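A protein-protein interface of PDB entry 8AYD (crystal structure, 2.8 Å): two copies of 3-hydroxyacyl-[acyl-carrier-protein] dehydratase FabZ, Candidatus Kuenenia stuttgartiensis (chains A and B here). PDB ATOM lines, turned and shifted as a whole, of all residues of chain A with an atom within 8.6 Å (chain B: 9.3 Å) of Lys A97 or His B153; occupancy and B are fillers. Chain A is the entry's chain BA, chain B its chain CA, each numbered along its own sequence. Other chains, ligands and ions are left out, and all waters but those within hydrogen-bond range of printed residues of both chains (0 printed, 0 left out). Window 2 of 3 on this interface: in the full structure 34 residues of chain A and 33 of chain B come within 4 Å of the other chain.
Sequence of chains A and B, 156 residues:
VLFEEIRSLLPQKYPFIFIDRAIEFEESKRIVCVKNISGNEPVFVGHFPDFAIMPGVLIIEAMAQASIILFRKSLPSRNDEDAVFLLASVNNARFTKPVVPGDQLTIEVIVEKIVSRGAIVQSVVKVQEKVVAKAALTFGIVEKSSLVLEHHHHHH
The guanidinium group (NH1) of Arg A94 is in hydrogen-bond range of the backbone carbonyl oxygen (O) of Ala B88 (2.5 Å).
The backbone NH (N) of Phe A95 sits at hydrogen-bond distance from the backbone carbonyl oxygen (O) of Ala B88.
The side-chain amino group (NZ) of Lys A97 is in hydrogen-bond range of a ring nitrogen (ND1) of His B153 (2.9 Å).
The side-chain carboxylate of Asp A103 is in hydrogen-bond range of the backbone NH of Val A100 (3.1 Å).
The backbone carbonyl oxygen of Leu B149 lies close to a ring nitrogen (NE2) of His B153, at 3.3 Å.
Ile A53 touches Leu B86 (CD1 to CD2, 3.8 Å).
Phe A95 touches Leu B87.
Val A100 touches Glu B150 (CG2 to OE2, 3.5 Å).
Val A100 touches His B154.
Asp A103 touches His B154.
Of the printed residues of chain B, Phe A95 touches Leu B87 and Ala B88.
No residue of chain B comes within 4 Å of Thr A96.
Of chain B, only His B153 comes within 4 Å of Lys A97.
No residue of chain B comes within 4 Å of Pro A98.
Printed residues of chain B within 4 Å of Val A100: Glu B150 (3.5 Å) and His B154 (3.5 Å).
Ala A133 touches none of the printed residues of chain B.
Of the printed residues of chain A, Leu B86 touches Ile A53 (3.8 Å).
Printed residues of chain A within 4 Å of Leu B87: Phe A95.
His B153 touches just one residue of chain A: Lys A97.
Of the printed residues of chain A, His B154 touches Val A100 and Asp A103.
Hydrophobic or aromatic side chains of chain A within 4 Å of the printed part of chain B: Ile A53, Phe A95 and Val A100.
Of the 13 printed residues of chain B, 6 touch a printed residue of chain A.
Hydrophobic or aromatic side chains of chain B within 4 Å of the printed part of chain A: Leu B86, Ala B88, His B153 and His B154.
Among the printed residues, 8 pairs touch across the chains.
Among the printed residues, no Asp or Glu carboxylate lies within 4 Å of a Lys or Arg side-chain nitrogen of the other chain.
No position is printed for both chains.
Of the 8 pairs that touch across the chains among the printed residues, none has its exchanged pair printed and touching as well.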
ATOM      1  N   PHE A  51     -17.789   9.112  -7.340  1.00  0.00           N
ATOM      2  CA  PHE A  51     -17.072   7.905  -7.753  1.00  0.00           C
ATOM      3  C   PHE A  51     -16.953   7.910  -9.273  1.00  0.00           C
ATOM      4  O   PHE A  51     -17.962   7.811  -9.974  1.00  0.00           O
ATOM      5  CB  PHE A  51     -17.790   6.665  -7.218  1.00  0.00           C
ATOM      6  CG  PHE A  51     -17.252   5.351  -7.722  1.00  0.00           C
ATOM      7  CD1 PHE A  51     -15.911   5.047  -7.631  1.00  0.00           C
ATOM      8  CD2 PHE A  51     -18.119   4.364  -8.150  1.00  0.00           C
ATOM      9  CE1 PHE A  51     -15.423   3.830  -8.067  1.00  0.00           C
ATOM     10  CE2 PHE A  51     -17.639   3.133  -8.568  1.00  0.00           C
ATOM     11  CZ  PHE A  51     -16.291   2.868  -8.530  1.00  0.00           C
ATOM     12  N   ILE A  53     -16.639   6.821 -12.730  1.00  0.00           N
ATOM     13  CA  ILE A  53     -16.846   5.667 -13.596  1.00  0.00           C
ATOM     14  C   ILE A  53     -16.992   6.173 -15.022  1.00  0.00           C
ATOM     15  O   ILE A  53     -17.653   7.189 -15.262  1.00  0.00           O
ATOM     16  CB  ILE A  53     -18.099   4.858 -13.201  1.00  0.00           C
ATOM     17  CG1 ILE A  53     -18.086   4.490 -11.723  1.00  0.00           C
ATOM     18  CG2 ILE A  53     -18.179   3.576 -14.011  1.00  0.00           C
ATOM     19  CD1 ILE A  53     -19.429   3.962 -11.265  1.00  0.00           C
ATOM     20  N   MET A  54     -16.384   5.467 -15.962  1.00  0.00           N
ATOM     21  CA  MET A  54     -16.606   5.758 -17.371  1.00  0.00           C
ATOM     22  C   MET A  54     -18.054   5.436 -17.718  1.00  0.00           C
ATOM     23  O   MET A  54     -18.479   4.286 -17.539  1.00  0.00           O
ATOM     24  CB  MET A  54     -15.649   4.942 -18.231  1.00  0.00           C
ATOM     25  CG  MET A  54     -15.630   5.285 -19.711  1.00  0.00           C
ATOM     26  SD  MET A  54     -14.900   6.898 -20.051  1.00  0.00           S
ATOM     27  CE  MET A  54     -15.545   7.222 -21.688  1.00  0.00           C
ATOM     28  N   PRO A  55     -18.846   6.403 -18.184  1.00  0.00           N
ATOM     29  CA  PRO A  55     -20.249   6.112 -18.502  1.00  0.00           C
ATOM     30  C   PRO A  55     -20.362   5.047 -19.580  1.00  0.00           C
ATOM     31  O   PRO A  55     -19.566   4.999 -20.520  1.00  0.00           O
ATOM     32  CB  PRO A  55     -20.790   7.463 -18.987  1.00  0.00           C
ATOM     33  CG  PRO A  55     -19.880   8.474 -18.376  1.00  0.00           C
ATOM     34  CD  PRO A  55     -18.525   7.828 -18.358  1.00  0.00           C
ATOM     35  N   GLY A  56     -21.363   4.180 -19.428  1.00  0.00           N
ATOM     36  CA  GLY A  56     -21.546   3.110 -20.393  1.00  0.00           C
ATOM     37  C   GLY A  56     -21.846   3.620 -21.787  1.00  0.00           C
ATOM     38  O   GLY A  56     -21.356   3.074 -22.778  1.00  0.00           O
ATOM     39  N   ILE A  59     -18.841   4.405 -23.755  1.00  0.00           N
ATOM     40  CA  ILE A  59     -18.158   3.230 -24.286  1.00  0.00           C
ATOM     41  C   ILE A  59     -18.753   2.846 -25.634  1.00  0.00           C
ATOM     42  O   ILE A  59     -18.039   2.397 -26.540  1.00  0.00           O
ATOM     43  CB  ILE A  59     -18.228   2.070 -23.275  1.00  0.00           C
ATOM     44  CG1 ILE A  59     -17.534   2.456 -21.969  1.00  0.00           C
ATOM     45  CG2 ILE A  59     -17.591   0.815 -23.853  1.00  0.00           C
ATOM     46  CD1 ILE A  59     -17.775   1.478 -20.840  1.00  0.00           C
ATOM     47  N   ARG A  94     -24.142  -5.194 -23.906  1.00  0.00           N
ATOM     48  CA  ARG A  94     -23.947  -5.784 -22.589  1.00  0.00           C
ATOM     49  C   ARG A  94     -22.735  -5.144 -21.934  1.00  0.00           C
ATOM     50  O   ARG A  94     -21.656  -5.108 -22.533  1.00  0.00           O
ATOM     51  CB  ARG A  94     -23.729  -7.295 -22.690  1.00  0.00           C
ATOM     52  CG  ARG A  94     -23.477  -7.949 -21.347  1.00  0.00           C
ATOM     53  CD  ARG A  94     -24.764  -8.098 -20.560  1.00  0.00           C
ATOM     54  NE  ARG A  94     -24.506  -8.464 -19.173  1.00  0.00           N
ATOM     55  CZ  ARG A  94     -24.434  -7.581 -18.182  1.00  0.00           C
ATOM     56  NH1 ARG A  94     -24.641  -6.292 -18.427  1.00  0.00           N
ATOM     57  NH2 ARG A  94     -24.187  -7.984 -16.944  1.00  0.00           N
ATOM     58  N   PHE A  95     -22.903  -4.625 -20.715  1.00  0.00           N
ATOM     59  CA  PHE A  95     -21.782  -4.027 -19.999  1.00  0.00           C
ATOM     60  C   PHE A  95     -21.689  -4.736 -18.656  1.00  0.00           C
ATOM     61  O   PHE A  95     -22.707  -4.920 -17.985  1.00  0.00           O
ATOM     62  CB  PHE A  95     -21.894  -2.499 -19.745  1.00  0.00           C
ATOM     63  CG  PHE A  95     -22.423  -1.663 -20.914  1.00  0.00           C
ATOM     64  CD1 PHE A  95     -23.326  -2.157 -21.843  1.00  0.00           C
ATOM     65  CD2 PHE A  95     -21.909  -0.400 -21.133  1.00  0.00           C
ATOM     66  CE1 PHE A  95     -23.780  -1.391 -22.885  1.00  0.00           C
ATOM     67  CE2 PHE A  95     -22.345   0.361 -22.198  1.00  0.00           C
ATOM     68  CZ  PHE A  95     -23.281  -0.135 -23.070  1.00  0.00           C
ATOM     69  N   THR A  96     -20.480  -5.129 -18.261  1.00  0.00           N
ATOM     70  CA  THR A  96     -20.293  -5.944 -17.062  1.00  0.00           C
ATOM     71  C   THR A  96     -19.543  -5.224 -15.963  1.00  0.00           C
ATOM     72  O   THR A  96     -20.060  -5.085 -14.846  1.00  0.00           O
ATOM     73  CB  THR A  96     -19.572  -7.251 -17.426  1.00  0.00           C
ATOM     74  OG1 THR A  96     -18.250  -6.952 -17.889  1.00  0.00           O
ATOM     75  CG2 THR A  96     -20.327  -7.995 -18.516  1.00  0.00           C
ATOM     76  N   LYS A  97     -18.319  -4.744 -16.230  1.00  0.00           N
ATOM     77  CA  LYS A  97     -17.474  -4.247 -15.157  1.00  0.00           C
ATOM     78  C   LYS A  97     -17.278  -2.739 -15.258  1.00  0.00           C
ATOM     79  O   LYS A  97     -17.124  -2.208 -16.363  1.00  0.00           O
ATOM     80  CB  LYS A  97     -16.099  -4.923 -15.180  1.00  0.00           C
ATOM     81  CG  LYS A  97     -16.128  -6.419 -14.922  1.00  0.00           C
ATOM     82  CD  LYS A  97     -14.721  -6.992 -14.888  1.00  0.00           C
ATOM     83  CE  LYS A  97     -14.745  -8.507 -14.786  1.00  0.00           C
ATOM     84  NZ  LYS A  97     -15.308  -8.981 -13.494  1.00  0.00           N
ATOM     85  N   PRO A  98     -17.274  -2.029 -14.130  1.00  0.00           N
ATOM     86  CA  PRO A  98     -16.958  -0.595 -14.164  1.00  0.00           C
ATOM     87  C   PRO A  98     -15.518  -0.374 -14.605  1.00  0.00           C
ATOM     88  O   PRO A  98     -14.592  -1.005 -14.089  1.00  0.00           O
ATOM     89  CB  PRO A  98     -17.177  -0.146 -12.713  1.00  0.00           C
ATOM     90  CG  PRO A  98     -18.086  -1.176 -12.129  1.00  0.00           C
ATOM     91  CD  PRO A  98     -17.695  -2.467 -12.789  1.00  0.00           C
ATOM     92  N   VAL A  99     -15.338   0.525 -15.567  1.00  0.00           N
ATOM     93  CA  VAL A  99     -14.018   0.924 -16.041  1.00  0.00           C
ATOM     94  C   VAL A  99     -13.722   2.318 -15.501  1.00  0.00           C
ATOM     95  O   VAL A  99     -14.546   3.232 -15.626  1.00  0.00           O
ATOM     96  CB  VAL A  99     -13.928   0.865 -17.576  1.00  0.00           C
ATOM     97  CG1 VAL A  99     -13.934  -0.578 -18.036  1.00  0.00           C
ATOM     98  CG2 VAL A  99     -15.103   1.572 -18.206  1.00  0.00           C
ATOM     99  N   VAL A 100     -12.554   2.469 -14.885  1.00  0.00           N
ATOM    100  CA  VAL A 100     -12.219   3.651 -14.093  1.00  0.00           C
ATOM    101  C   VAL A 100     -10.965   4.313 -14.656  1.00  0.00           C
ATOM    102  O   VAL A 100     -10.298   3.725 -15.520  1.00  0.00           O
ATOM    103  CB  VAL A 100     -12.034   3.273 -12.614  1.00  0.00           C
ATOM    104  CG1 VAL A 100     -13.341   2.764 -12.030  1.00  0.00           C
ATOM    105  CG2 VAL A 100     -10.941   2.224 -12.474  1.00  0.00           C
ATOM    106  N   ASP A 103      -7.379   2.665 -16.549  1.00  0.00           N
ATOM    107  CA  ASP A 103      -7.574   1.526 -17.432  1.00  0.00           C
ATOM    108  C   ASP A 103      -7.353   1.919 -18.887  1.00  0.00           C
ATOM    109  O   ASP A 103      -7.538   3.076 -19.276  1.00  0.00           O
ATOM    110  CB  ASP A 103      -8.986   0.954 -17.267  1.00  0.00           C
ATOM    111  CG  ASP A 103      -9.206   0.324 -15.907  1.00  0.00           C
ATOM    112  OD1 ASP A 103      -8.226  -0.173 -15.313  1.00  0.00           O
ATOM    113  OD2 ASP A 103     -10.362   0.325 -15.431  1.00  0.00           O
ATOM    114  N   LEU A 105      -8.788   0.855 -22.669  1.00  0.00           N
ATOM    115  CA  LEU A 105      -9.842   0.173 -23.406  1.00  0.00           C
ATOM    116  C   LEU A 105      -9.296  -0.230 -24.770  1.00  0.00           C
ATOM    117  O   LEU A 105      -8.938   0.633 -25.579  1.00  0.00           O
ATOM    118  CB  LEU A 105     -11.071   1.069 -23.563  1.00  0.00           C
ATOM    119  CG  LEU A 105     -11.797   1.473 -22.279  1.00  0.00           C
ATOM    120  CD1 LEU A 105     -12.938   2.432 -22.592  1.00  0.00           C
ATOM    121  CD2 LEU A 105     -12.302   0.252 -21.527  1.00  0.00           C
ATOM    122  N   VAL A 125     -15.283  -4.506 -26.341  1.00  0.00           N
ATOM    123  CA  VAL A 125     -14.310  -3.680 -25.636  1.00  0.00           C
ATOM    124  C   VAL A 125     -13.763  -4.478 -24.462  1.00  0.00           C
ATOM    125  O   VAL A 125     -14.506  -5.212 -23.798  1.00  0.00           O
ATOM    126  CB  VAL A 125     -14.934  -2.352 -25.161  1.00  0.00           C
ATOM    127  CG1 VAL A 125     -13.932  -1.539 -24.353  1.00  0.00           C
ATOM    128  CG2 VAL A 125     -15.428  -1.550 -26.349  1.00  0.00           C
ATOM    129  N   VAL A 127     -10.739  -4.584 -21.068  1.00  0.00           N
ATOM    130  CA  VAL A 127      -9.638  -4.156 -20.217  1.00  0.00           C
ATOM    131  C   VAL A 127      -8.739  -5.382 -20.258  1.00  0.00           C
ATOM    132  O   VAL A 127      -9.129  -6.396 -20.843  1.00  0.00           O
ATOM    133  CB  VAL A 127     -10.098  -3.764 -18.799  1.00  0.00           C
ATOM    134  CG1 VAL A 127      -8.939  -3.220 -17.957  1.00  0.00           C
ATOM    135  CG2 VAL A 127     -11.204  -2.731 -18.881  1.00  0.00           C
ATOM    136  N   GLN A 128      -7.582  -5.336 -19.597  1.00  0.00           N
ATOM    137  CA  GLN A 128      -6.329  -5.941 -20.041  1.00  0.00           C
ATOM    138  C   GLN A 128      -6.526  -7.161 -20.939  1.00  0.00           C
ATOM    139  O   GLN A 128      -5.968  -7.206 -22.041  1.00  0.00           O
ATOM    140  CB  GLN A 128      -5.521  -6.325 -18.802  1.00  0.00           C
ATOM    141  CG  GLN A 128      -5.510  -5.217 -17.753  1.00  0.00           C
ATOM    142  CD  GLN A 128      -4.731  -5.583 -16.509  1.00  0.00           C
ATOM    143  OE1 GLN A 128      -4.056  -6.612 -16.466  1.00  0.00           O
ATOM    144  NE2 GLN A 128      -4.876  -4.772 -15.462  1.00  0.00           N
ATOM    145  N   GLU A 129      -7.311  -8.157 -20.505  1.00  0.00           N
ATOM    146  CA  GLU A 129      -7.933  -9.063 -21.465  1.00  0.00           C
ATOM    147  C   GLU A 129      -9.336  -9.498 -21.048  1.00  0.00           C
ATOM    148  O   GLU A 129      -9.960 -10.284 -21.768  1.00  0.00           O
ATOM    149  CB  GLU A 129      -7.042 -10.295 -21.720  1.00  0.00           C
ATOM    150  CG  GLU A 129      -7.366 -11.020 -23.030  1.00  0.00           C
ATOM    151  CD  GLU A 129      -7.076 -10.152 -24.251  1.00  0.00           C
ATOM    152  OE1 GLU A 129      -6.174  -9.292 -24.169  1.00  0.00           O
ATOM    153  OE2 GLU A 129      -7.757 -10.314 -25.287  1.00  0.00           O
ATOM    154  N   LYS A 130      -9.863  -8.997 -19.929  1.00  0.00           N
ATOM    155  CA  LYS A 130     -11.221  -9.320 -19.502  1.00  0.00           C
ATOM    156  C   LYS A 130     -12.234  -8.435 -20.218  1.00  0.00           C
ATOM    157  O   LYS A 130     -12.083  -7.209 -20.258  1.00  0.00           O
ATOM    158  CB  LYS A 130     -11.356  -9.165 -17.985  1.00  0.00           C
ATOM    159  CG  LYS A 130     -10.684 -10.270 -17.182  1.00  0.00           C
ATOM    160  CD  LYS A 130     -11.484 -11.569 -17.248  1.00  0.00           C
ATOM    161  CE  LYS A 130     -12.667 -11.551 -16.286  1.00  0.00           C
ATOM    162  NZ  LYS A 130     -12.192 -11.616 -14.868  1.00  0.00           N
ATOM    163  N   VAL A 131     -13.269  -9.062 -20.781  1.00  0.00           N
ATOM    164  CA  VAL A 131     -14.292  -8.335 -21.525  1.00  0.00           C
ATOM    165  C   VAL A 131     -15.141  -7.519 -20.562  1.00  0.00           C
ATOM    166  O   VAL A 131     -15.604  -8.026 -19.530  1.00  0.00           O
ATOM    167  CB  VAL A 131     -15.158  -9.312 -22.335  1.00  0.00           C
ATOM    168  CG1 VAL A 131     -16.277  -8.572 -23.057  1.00  0.00           C
ATOM    169  CG2 VAL A 131     -14.302 -10.095 -23.318  1.00  0.00           C
ATOM    170  N   VAL A 132     -15.359  -6.248 -20.895  1.00  0.00           N
ATOM    171  CA  VAL A 132     -16.165  -5.366 -20.063  1.00  0.00           C
ATOM    172  C   VAL A 132     -17.352  -4.762 -20.801  1.00  0.00           C
ATOM    173  O   VAL A 132     -18.279  -4.263 -20.144  1.00  0.00           O
ATOM    174  CB  VAL A 132     -15.304  -4.245 -19.442  1.00  0.00           C
ATOM    175  CG1 VAL A 132     -14.245  -4.835 -18.525  1.00  0.00           C
ATOM    176  CG2 VAL A 132     -14.666  -3.398 -20.534  1.00  0.00           C
ATOM    177  N   ALA A 133     -17.370  -4.780 -22.133  1.00  0.00           N
ATOM    178  CA  ALA A 133     -18.481  -4.217 -22.887  1.00  0.00           C
ATOM    179  C   ALA A 133     -18.482  -4.805 -24.291  1.00  0.00           C
ATOM    180  O   ALA A 133     -17.420  -5.008 -24.885  1.00  0.00           O
ATOM    181  CB  ALA A 133     -18.394  -2.687 -22.955  1.00  0.00           C
ATOM    182  N   LEU B  86     -25.988   1.296 -12.582  1.00  0.00           N
ATOM    183  CA  LEU B  86     -25.100   1.303 -13.733  1.00  0.00           C
ATOM    184  C   LEU B  86     -25.757   0.623 -14.927  1.00  0.00           C
ATOM    185  O   LEU B  86     -26.497  -0.352 -14.778  1.00  0.00           O
ATOM    186  CB  LEU B  86     -23.774   0.623 -13.393  1.00  0.00           C
ATOM    187  CG  LEU B  86     -23.002   1.337 -12.279  1.00  0.00           C
ATOM    188  CD1 LEU B  86     -21.695   0.620 -11.975  1.00  0.00           C
ATOM    189  CD2 LEU B  86     -22.766   2.812 -12.602  1.00  0.00           C
ATOM    190  N   LEU B  87     -25.482   1.153 -16.115  1.00  0.00           N
ATOM    191  CA  LEU B  87     -26.143   0.697 -17.331  1.00  0.00           C
ATOM    192  C   LEU B  87     -25.604  -0.677 -17.717  1.00  0.00           C
ATOM    193  O   LEU B  87     -24.394  -0.847 -17.900  1.00  0.00           O
ATOM    194  CB  LEU B  87     -25.924   1.713 -18.448  1.00  0.00           C
ATOM    195  CG  LEU B  87     -26.733   1.580 -19.735  1.00  0.00           C
ATOM    196  CD1 LEU B  87     -28.214   1.744 -19.434  1.00  0.00           C
ATOM    197  CD2 LEU B  87     -26.276   2.614 -20.749  1.00  0.00           C
ATOM    198  N   ALA B  88     -26.497  -1.659 -17.831  1.00  0.00           N
ATOM    199  CA  ALA B  88     -26.095  -3.050 -17.992  1.00  0.00           C
ATOM    200  C   ALA B  88     -26.530  -3.684 -19.304  1.00  0.00           C
ATOM    201  O   ALA B  88     -25.844  -4.587 -19.784  1.00  0.00           O
ATOM    202  CB  ALA B  88     -26.639  -3.900 -16.833  1.00  0.00           C
ATOM    203  N   SER B 145     -20.808  -1.375  -1.850  1.00  0.00           N
ATOM    204  CA  SER B 145     -20.213  -2.666  -2.171  1.00  0.00           C
ATOM    205  C   SER B 145     -19.552  -2.619  -3.543  1.00  0.00           C
ATOM    206  O   SER B 145     -18.631  -3.387  -3.819  1.00  0.00           O
ATOM    207  CB  SER B 145     -21.277  -3.763  -2.133  1.00  0.00           C
ATOM    208  OG  SER B 145     -22.242  -3.562  -3.151  1.00  0.00           O
ATOM    209  N   SER B 146     -20.015  -1.710  -4.405  1.00  0.00           N
ATOM    210  CA  SER B 146     -19.479  -1.569  -5.756  1.00  0.00           C
ATOM    211  C   SER B 146     -18.005  -1.182  -5.763  1.00  0.00           C
ATOM    212  O   SER B 146     -17.301  -1.457  -6.742  1.00  0.00           O
ATOM    213  CB  SER B 146     -20.293  -0.527  -6.529  1.00  0.00           C
ATOM    214  OG  SER B 146     -19.762  -0.313  -7.822  1.00  0.00           O
ATOM    215  N   LEU B 147     -17.522  -0.525  -4.707  1.00  0.00           N
ATOM    216  CA  LEU B 147     -16.121  -0.109  -4.681  1.00  0.00           C
ATOM    217  C   LEU B 147     -15.195  -1.311  -4.549  1.00  0.00           C
ATOM    218  O   LEU B 147     -14.281  -1.501  -5.361  1.00  0.00           O
ATOM    219  CB  LEU B 147     -15.876   0.881  -3.544  1.00  0.00           C
ATOM    220  CG  LEU B 147     -16.264   2.337  -3.808  1.00  0.00           C
ATOM    221  CD1 LEU B 147     -17.768   2.533  -3.746  1.00  0.00           C
ATOM    222  CD2 LEU B 147     -15.560   3.253  -2.834  1.00  0.00           C
ATOM    223  N   VAL B 148     -15.411  -2.134  -3.521  1.00  0.00           N
ATOM    224  CA  VAL B 148     -14.575  -3.316  -3.333  1.00  0.00           C
ATOM    225  C   VAL B 148     -14.734  -4.285  -4.495  1.00  0.00           C
ATOM    226  O   VAL B 148     -13.790  -5.008  -4.840  1.00  0.00           O
ATOM    227  CB  VAL B 148     -14.890  -3.982  -1.981  1.00  0.00           C
ATOM    228  CG1 VAL B 148     -14.456  -3.080  -0.840  1.00  0.00           C
ATOM    229  CG2 VAL B 148     -16.365  -4.255  -1.879  1.00  0.00           C
ATOM    230  N   LEU B 149     -15.914  -4.325  -5.119  1.00  0.00           N
ATOM    231  CA  LEU B 149     -16.053  -5.080  -6.360  1.00  0.00           C
ATOM    232  C   LEU B 149     -15.085  -4.550  -7.407  1.00  0.00           C
ATOM    233  O   LEU B 149     -14.259  -5.297  -7.943  1.00  0.00           O
ATOM    234  CB  LEU B 149     -17.494  -5.009  -6.870  1.00  0.00           C
ATOM    235  CG  LEU B 149     -18.591  -5.598  -5.977  1.00  0.00           C
ATOM    236  CD1 LEU B 149     -19.969  -5.406  -6.607  1.00  0.00           C
ATOM    237  CD2 LEU B 149     -18.332  -7.060  -5.643  1.00  0.00           C
ATOM    238  N   GLU B 150     -15.157  -3.244  -7.684  1.00  0.00           N
ATOM    239  CA  GLU B 150     -14.181  -2.588  -8.546  1.00  0.00           C
ATOM    240  C   GLU B 150     -12.759  -2.757  -8.021  1.00  0.00           C
ATOM    241  O   GLU B 150     -11.808  -2.804  -8.811  1.00  0.00           O
ATOM    242  CB  GLU B 150     -14.553  -1.110  -8.692  1.00  0.00           C
ATOM    243  CG  GLU B 150     -13.653  -0.282  -9.592  1.00  0.00           C
ATOM    244  CD  GLU B 150     -12.555   0.419  -8.815  1.00  0.00           C
ATOM    245  OE1 GLU B 150     -12.788   0.748  -7.633  1.00  0.00           O
ATOM    246  OE2 GLU B 150     -11.467   0.644  -9.384  1.00  0.00           O
ATOM    247  N   HIS B 151     -12.590  -2.860  -6.701  1.00  0.00           N
ATOM    248  CA  HIS B 151     -11.281  -3.196  -6.150  1.00  0.00           C
ATOM    249  C   HIS B 151     -10.883  -4.627  -6.491  1.00  0.00           C
ATOM    250  O   HIS B 151      -9.719  -4.889  -6.815  1.00  0.00           O
ATOM    251  CB  HIS B 151     -11.274  -2.990  -4.636  1.00  0.00           C
ATOM    252  CG  HIS B 151      -9.978  -3.357  -3.983  1.00  0.00           C
ATOM    253  ND1 HIS B 151      -9.700  -4.637  -3.555  1.00  0.00           N
ATOM    254  CD2 HIS B 151      -8.882  -2.617  -3.690  1.00  0.00           C
ATOM    255  CE1 HIS B 151      -8.491  -4.670  -3.023  1.00  0.00           C
ATOM    256  NE2 HIS B 151      -7.973  -3.457  -3.093  1.00  0.00           N
ATOM    257  N   HIS B 152     -11.829  -5.566  -6.421  1.00  0.00           N
ATOM    258  CA  HIS B 152     -11.492  -6.960  -6.688  1.00  0.00           C
ATOM    259  C   HIS B 152     -11.184  -7.199  -8.161  1.00  0.00           C
ATOM    260  O   HIS B 152     -10.443  -8.132  -8.489  1.00  0.00           O
ATOM    261  CB  HIS B 152     -12.619  -7.886  -6.229  1.00  0.00           C
ATOM    262  CG  HIS B 152     -12.803  -7.927  -4.744  1.00  0.00           C
ATOM    263  ND1 HIS B 152     -13.687  -7.104  -4.080  1.00  0.00           N
ATOM    264  CD2 HIS B 152     -12.205  -8.681  -3.791  1.00  0.00           C
ATOM    265  CE1 HIS B 152     -13.633  -7.355  -2.785  1.00  0.00           C
ATOM    266  NE2 HIS B 152     -12.742  -8.308  -2.582  1.00  0.00           N
ATOM    267  N   HIS B 153     -11.732  -6.376  -9.060  1.00  0.00           N
ATOM    268  CA  HIS B 153     -11.432  -6.554 -10.476  1.00  0.00           C
ATOM    269  C   HIS B 153     -10.000  -6.165 -10.818  1.00  0.00           C
ATOM    270  O   HIS B 153      -9.525  -6.511 -11.905  1.00  0.00           O
ATOM    271  CB  HIS B 153     -12.382  -5.731 -11.351  1.00  0.00           C
ATOM    272  CG  HIS B 153     -13.834  -5.992 -11.098  1.00  0.00           C
ATOM    273  ND1 HIS B 153     -14.421  -7.221 -11.306  1.00  0.00           N
ATOM    274  CD2 HIS B 153     -14.832  -5.159 -10.720  1.00  0.00           C
ATOM    275  CE1 HIS B 153     -15.708  -7.146 -11.017  1.00  0.00           C
ATOM    276  NE2 HIS B 153     -15.984  -5.904 -10.662  1.00  0.00           N
ATOM    277  N   HIS B 154      -9.310  -5.461  -9.925  1.00  0.00           N
ATOM    278  CA  HIS B 154      -7.992  -4.916 -10.218  1.00  0.00           C
ATOM    279  C   HIS B 154      -6.933  -5.473  -9.273  1.00  0.00           C
ATOM    280  O   HIS B 154      -7.168  -5.605  -8.072  1.00  0.00           O
ATOM    281  CB  HIS B 154      -8.028  -3.389 -10.130  1.00  0.00           C
ATOM    282  CG  HIS B 154      -8.878  -2.745 -11.181  1.00  0.00           C
ATOM    283  ND1 HIS B 154      -9.224  -1.412 -11.144  1.00  0.00           N
ATOM    284  CD2 HIS B 154      -9.447  -3.251 -12.299  1.00  0.00           C
ATOM    285  CE1 HIS B 154      -9.975  -1.125 -12.193  1.00  0.00           C
ATOM    286  NE2 HIS B 154     -10.125  -2.224 -12.910  1.00  0.00           N
